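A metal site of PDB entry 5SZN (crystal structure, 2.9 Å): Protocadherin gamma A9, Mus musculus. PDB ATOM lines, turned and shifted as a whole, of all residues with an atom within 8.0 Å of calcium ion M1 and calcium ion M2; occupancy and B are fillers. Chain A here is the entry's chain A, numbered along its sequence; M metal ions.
The guanidinium group (NH1) of Arg 64 sits close to the side-chain carboxylate (OE2) of Glu 65. The side-chain carboxylate (OD2) of Asp 133 sits close to the side-chain amide oxygen (OD1) of Asn 99 (2.9 Å). N of Glu 10 is in hydrogen-bond range of O of Ile 62, 2.4 Å away. The side-chain amide nitrogen (ND2) of Asn 137 is in hydrogen-bond range of the side-chain carboxylate (OD2) of Asp 97. The side-chain carboxylate (OD2) of Asp 63 sits at hydrogen-bond distance from the backbone NH (N) of Glu 66 (2.7 Å). OD1 of Asp 97 is in salt-bridge range of NE of Arg 64, 3.9 Å away. The side-chain carboxylate of Asp 100 lies close to the side-chain amide nitrogen of Asn 101 (3.0 Å).
Merely in contact with calcium ion M2: Asp 97. Within 4 Å of calcium ion M2: Glu 9, Glu 65, Asp 97, Ile 98, Asp 100 and Asp 133. The nearest printed residue that does not touch calcium ion M2 is Arg 64 (4.7 Å).
ND2 of Asn 101 touches calcium ion M1, 3.7 Å away. Of the 19 residues printed, 6 come within 4 Å of calcium ion M1.
Calcium ion M1 is bound by OE1 of Glu 65. Calcium ion M1 is bound by the side-chain carboxylate (OD1) of Asp 63 (2.4 Å). Calcium ion M1 is bound by OD2 of Asp 100 (2.5 Å). Calcium ion M1 has three donor atoms within binding distance. Slightly farther from calcium ion M1 lies OD1 of Asp 100 (2.9 Å). Slightly farther from calcium ion M1 lies OE1 of Glu 9 (3.0 Å). Slightly farther from calcium ion M1 lies OE2 of Glu 10 (3.1 Å).
Calcium ion M2 is bound by the side-chain carboxylate of Glu 9, the side-chain carboxylate of Asp 100, the side-chain carboxylate of Glu 65, the backbone carbonyl oxygen of Ile 98 and the side-chain carboxylate of Asp 133. Calcium ion M2 has five donor atoms within binding distance.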
ATOM      1  N   GLU A   9      -2.930  15.865  11.501  1.00  0.00           N
ATOM      2  CA  GLU A   9      -4.016  16.632  10.931  1.00  0.00           C
ATOM      3  C   GLU A   9      -4.804  15.801   9.926  1.00  0.00           C
ATOM      4  O   GLU A   9      -4.301  14.817   9.362  1.00  0.00           O
ATOM      5  CB  GLU A   9      -3.490  17.888  10.235  1.00  0.00           C
ATOM      6  CG  GLU A   9      -2.478  17.592   9.148  1.00  0.00           C
ATOM      7  CD  GLU A   9      -2.275  18.769   8.209  1.00  0.00           C
ATOM      8  OE1 GLU A   9      -3.225  19.546   8.003  1.00  0.00           O
ATOM      9  OE2 GLU A   9      -1.146  18.910   7.695  1.00  0.00           O
ATOM     10  N   GLU A  10      -6.044  16.216   9.698  1.00  0.00           N
ATOM     11  CA  GLU A  10      -6.938  15.590   8.728  1.00  0.00           C
ATOM     12  C   GLU A  10      -7.040  14.085   8.935  1.00  0.00           C
ATOM     13  O   GLU A  10      -6.927  13.279   8.012  1.00  0.00           O
ATOM     14  CB  GLU A  10      -6.504  15.925   7.300  1.00  0.00           C
ATOM     15  CG  GLU A  10      -6.657  17.391   6.951  1.00  0.00           C
ATOM     16  CD  GLU A  10      -6.370  17.664   5.491  1.00  0.00           C
ATOM     17  OE1 GLU A  10      -5.818  16.775   4.816  1.00  0.00           O
ATOM     18  OE2 GLU A  10      -6.690  18.779   5.022  1.00  0.00           O
ATOM     19  N   ILE A  62      -9.479  17.833  11.229  1.00  0.00           N
ATOM     20  CA  ILE A  62      -8.605  18.945  11.604  1.00  0.00           C
ATOM     21  C   ILE A  62      -7.730  19.296  10.416  1.00  0.00           C
ATOM     22  O   ILE A  62      -6.956  18.466   9.932  1.00  0.00           O
ATOM     23  CB  ILE A  62      -7.722  18.595  12.818  1.00  0.00           C
ATOM     24  CG1 ILE A  62      -8.575  18.289  14.044  1.00  0.00           C
ATOM     25  CG2 ILE A  62      -6.752  19.730  13.113  1.00  0.00           C
ATOM     26  CD1 ILE A  62      -8.745  16.820  14.310  1.00  0.00           C
ATOM     27  N   ASP A  63      -7.840  20.538   9.953  1.00  0.00           N
ATOM     28  CA  ASP A  63      -6.966  21.071   8.910  1.00  0.00           C
ATOM     29  C   ASP A  63      -6.280  22.306   9.491  1.00  0.00           C
ATOM     30  O   ASP A  63      -6.851  23.391   9.519  1.00  0.00           O
ATOM     31  CB  ASP A  63      -7.737  21.413   7.643  1.00  0.00           C
ATOM     32  CG  ASP A  63      -6.883  22.093   6.590  1.00  0.00           C
ATOM     33  OD1 ASP A  63      -6.149  21.381   5.872  1.00  0.00           O
ATOM     34  OD2 ASP A  63      -6.938  23.333   6.496  1.00  0.00           O
ATOM     35  N   ARG A  64      -5.035  22.125   9.960  1.00  0.00           N
ATOM     36  CA  ARG A  64      -4.311  23.214  10.595  1.00  0.00           C
ATOM     37  C   ARG A  64      -4.037  24.370   9.630  1.00  0.00           C
ATOM     38  O   ARG A  64      -3.738  25.483  10.083  1.00  0.00           O
ATOM     39  CB  ARG A  64      -2.994  22.712  11.186  1.00  0.00           C
ATOM     40  CG  ARG A  64      -2.180  21.846  10.244  1.00  0.00           C
ATOM     41  CD  ARG A  64      -0.732  21.787  10.682  1.00  0.00           C
ATOM     42  NE  ARG A  64      -0.170  23.123  10.801  1.00  0.00           N
ATOM     43  CZ  ARG A  64       0.300  23.838   9.786  1.00  0.00           C
ATOM     44  NH1 ARG A  64       0.263  23.341   8.550  1.00  0.00           N
ATOM     45  NH2 ARG A  64       0.793  25.049   9.987  1.00  0.00           N
ATOM     46  N   GLU A  65      -4.132  24.127   8.318  1.00  0.00           N
ATOM     47  CA  GLU A  65      -4.050  25.225   7.365  1.00  0.00           C
ATOM     48  C   GLU A  65      -5.232  26.171   7.517  1.00  0.00           C
ATOM     49  O   GLU A  65      -5.100  27.373   7.289  1.00  0.00           O
ATOM     50  CB  GLU A  65      -3.967  24.680   5.938  1.00  0.00           C
ATOM     51  CG  GLU A  65      -2.656  24.017   5.574  1.00  0.00           C
ATOM     52  CD  GLU A  65      -2.433  22.704   6.300  1.00  0.00           C
ATOM     53  OE1 GLU A  65      -3.426  22.109   6.780  1.00  0.00           O
ATOM     54  OE2 GLU A  65      -1.275  22.255   6.397  1.00  0.00           O
ATOM     55  N   GLU A  66      -6.402  25.642   7.885  1.00  0.00           N
ATOM     56  CA  GLU A  66      -7.565  26.442   8.219  1.00  0.00           C
ATOM     57  C   GLU A  66      -7.611  26.826   9.691  1.00  0.00           C
ATOM     58  O   GLU A  66      -8.637  27.339  10.152  1.00  0.00           O
ATOM     59  CB  GLU A  66      -8.850  25.706   7.826  1.00  0.00           C
ATOM     60  N   ALA A  69      -2.729  28.251   9.702  1.00  0.00           N
ATOM     61  CA  ALA A  69      -2.215  28.690   8.412  1.00  0.00           C
ATOM     62  C   ALA A  69      -0.727  28.382   8.252  1.00  0.00           C
ATOM     63  O   ALA A  69      -0.352  27.242   7.966  1.00  0.00           O
ATOM     64  CB  ALA A  69      -2.478  30.177   8.206  1.00  0.00           C
ATOM     65  N   VAL A  96       0.210  18.168  14.255  1.00  0.00           N
ATOM     66  CA  VAL A  96       1.382  18.079  13.385  1.00  0.00           C
ATOM     67  C   VAL A  96       0.940  18.356  11.964  1.00  0.00           C
ATOM     68  O   VAL A  96      -0.257  18.386  11.671  1.00  0.00           O
ATOM     69  CB  VAL A  96       2.080  16.711  13.501  1.00  0.00           C
ATOM     70  CG1 VAL A  96       2.201  16.299  14.960  1.00  0.00           C
ATOM     71  CG2 VAL A  96       1.336  15.670  12.694  1.00  0.00           C
ATOM     72  N   ASP A  97       1.894  18.564  11.060  1.00  0.00           N
ATOM     73  CA  ASP A  97       1.604  18.869   9.670  1.00  0.00           C
ATOM     74  C   ASP A  97       1.931  17.677   8.788  1.00  0.00           C
ATOM     75  O   ASP A  97       2.977  17.036   8.947  1.00  0.00           O
ATOM     76  CB  ASP A  97       2.383  20.096   9.200  1.00  0.00           C
ATOM     77  CG  ASP A  97       2.025  20.514   7.783  1.00  0.00           C
ATOM     78  OD1 ASP A  97       1.067  21.309   7.627  1.00  0.00           O
ATOM     79  OD2 ASP A  97       2.686  20.056   6.830  1.00  0.00           O
ATOM     80  N   ILE A  98       1.019  17.379   7.864  1.00  0.00           N
ATOM     81  CA  ILE A  98       1.244  16.382   6.824  1.00  0.00           C
ATOM     82  C   ILE A  98       1.159  17.084   5.472  1.00  0.00           C
ATOM     83  O   ILE A  98       0.547  18.149   5.342  1.00  0.00           O
ATOM     84  CB  ILE A  98       0.252  15.208   6.898  1.00  0.00           C
ATOM     85  CG1 ILE A  98      -1.152  15.661   6.479  1.00  0.00           C
ATOM     86  CG2 ILE A  98       0.231  14.618   8.307  1.00  0.00           C
ATOM     87  CD1 ILE A  98      -2.210  14.598   6.631  1.00  0.00           C
ATOM     88  N   ASN A  99       1.785  16.473   4.475  1.00  0.00           N
ATOM     89  CA  ASN A  99       1.848  17.060   3.136  1.00  0.00           C
ATOM     90  C   ASN A  99       0.645  16.591   2.333  1.00  0.00           C
ATOM     91  O   ASN A  99       0.662  15.517   1.719  1.00  0.00           O
ATOM     92  CB  ASN A  99       3.156  16.715   2.443  1.00  0.00           C
ATOM     93  CG  ASN A  99       3.290  17.388   1.090  1.00  0.00           C
ATOM     94  OD1 ASN A  99       2.813  18.505   0.895  1.00  0.00           O
ATOM     95  ND2 ASN A  99       3.928  16.702   0.151  1.00  0.00           N
ATOM     96  N   ASP A 100      -0.417  17.390   2.328  1.00  0.00           N
ATOM     97  CA  ASP A 100      -1.576  17.140   1.501  1.00  0.00           C
ATOM     98  C   ASP A 100      -1.843  18.229   0.475  1.00  0.00           C
ATOM     99  O   ASP A 100      -2.526  17.967  -0.518  1.00  0.00           O
ATOM    100  CB  ASP A 100      -2.840  16.976   2.377  1.00  0.00           C
ATOM    101  CG  ASP A 100      -3.077  18.170   3.273  1.00  0.00           C
ATOM    102  OD1 ASP A 100      -2.096  18.717   3.808  1.00  0.00           O
ATOM    103  OD2 ASP A 100      -4.246  18.583   3.434  1.00  0.00           O
ATOM    104  N   ASN A 101      -1.331  19.439   0.687  1.00  0.00           N
ATOM    105  CA  ASN A 101      -1.569  20.569  -0.205  1.00  0.00           C
ATOM    106  C   ASN A 101      -0.418  20.696  -1.192  1.00  0.00           C
ATOM    107  O   ASN A 101       0.755  20.561  -0.831  1.00  0.00           O
ATOM    108  CB  ASN A 101      -1.708  21.868   0.594  1.00  0.00           C
ATOM    109  CG  ASN A 101      -3.056  21.977   1.293  1.00  0.00           C
ATOM    110  OD1 ASN A 101      -3.544  23.080   1.549  1.00  0.00           O
ATOM    111  ND2 ASN A 101      -3.662  20.841   1.594  1.00  0.00           N
ATOM    112  N   ASP A 131       2.768  27.487  -0.764  1.00  0.00           N
ATOM    113  CA  ASP A 131       2.356  26.178  -0.295  1.00  0.00           C
ATOM    114  C   ASP A 131       1.788  26.342   1.112  1.00  0.00           C
ATOM    115  O   ASP A 131       2.506  26.827   2.015  1.00  0.00           O
ATOM    116  CB  ASP A 131       3.529  25.196  -0.305  1.00  0.00           C
ATOM    117  CG  ASP A 131       3.105  23.777   0.042  1.00  0.00           C
ATOM    118  OD1 ASP A 131       1.901  23.479   0.004  1.00  0.00           O
ATOM    119  OD2 ASP A 131       3.997  22.947   0.333  1.00  0.00           O
ATOM    120  N   PRO A 132       0.523  25.976   1.345  1.00  0.00           N
ATOM    121  CA  PRO A 132      -0.066  26.164   2.688  1.00  0.00           C
ATOM    122  C   PRO A 132       0.655  25.415   3.797  1.00  0.00           C
ATOM    123  O   PRO A 132       0.555  25.823   4.954  1.00  0.00           O
ATOM    124  CB  PRO A 132      -1.500  25.657   2.511  1.00  0.00           C
ATOM    125  CG  PRO A 132      -1.779  25.804   1.058  1.00  0.00           C
ATOM    126  CD  PRO A 132      -0.479  25.532   0.357  1.00  0.00           C
ATOM    127  N   ASP A 133       1.382  24.344   3.480  1.00  0.00           N
ATOM    128  CA  ASP A 133       2.046  23.550   4.497  1.00  0.00           C
ATOM    129  C   ASP A 133       3.224  24.321   5.092  1.00  0.00           C
ATOM    130  O   ASP A 133       3.575  25.426   4.668  1.00  0.00           O
ATOM    131  CB  ASP A 133       2.495  22.212   3.912  1.00  0.00           C
ATOM    132  CG  ASP A 133       1.345  21.414   3.339  1.00  0.00           C
ATOM    133  OD1 ASP A 133       0.236  21.478   3.901  1.00  0.00           O
ATOM    134  OD2 ASP A 133       1.542  20.727   2.309  1.00  0.00           O
ATOM    135  N   VAL A 134       3.848  23.720   6.114  1.00  0.00           N
ATOM    136  CA  VAL A 134       4.945  24.340   6.848  1.00  0.00           C
ATOM    137  C   VAL A 134       6.076  23.328   6.996  1.00  0.00           C
ATOM    138  O   VAL A 134       5.823  22.138   7.213  1.00  0.00           O
ATOM    139  CB  VAL A 134       4.479  24.845   8.235  1.00  0.00           C
ATOM    140  CG1 VAL A 134       5.645  25.390   9.036  1.00  0.00           C
ATOM    141  CG2 VAL A 134       3.389  25.893   8.090  1.00  0.00           C
ATOM    142  N   ASN A 137       7.095  19.886   4.434  1.00  0.00           N
ATOM    143  CA  ASN A 137       5.903  19.757   3.597  1.00  0.00           C
ATOM    144  C   ASN A 137       5.626  21.018   2.783  1.00  0.00           C
ATOM    145  O   ASN A 137       4.843  20.950   1.821  1.00  0.00           O
ATOM    146  CB  ASN A 137       4.690  19.427   4.467  1.00  0.00           C
ATOM    147  CG  ASN A 137       4.892  18.167   5.287  1.00  0.00           C
ATOM    148  OD1 ASN A 137       5.642  17.270   4.910  1.00  0.00           O
ATOM    149  ND2 ASN A 137       4.214  18.088   6.431  1.00  0.00           N
HETATM  150 CA    CA M   1      -4.046  20.324   5.252  1.00  0.00          CA
HETATM  151 CA    CA M   2      -1.216  19.986   5.605  1.00  0.00          CA
HETATM  152 CA    CA M   3       3.102  20.963  -0.175  1.00  0.00          CA
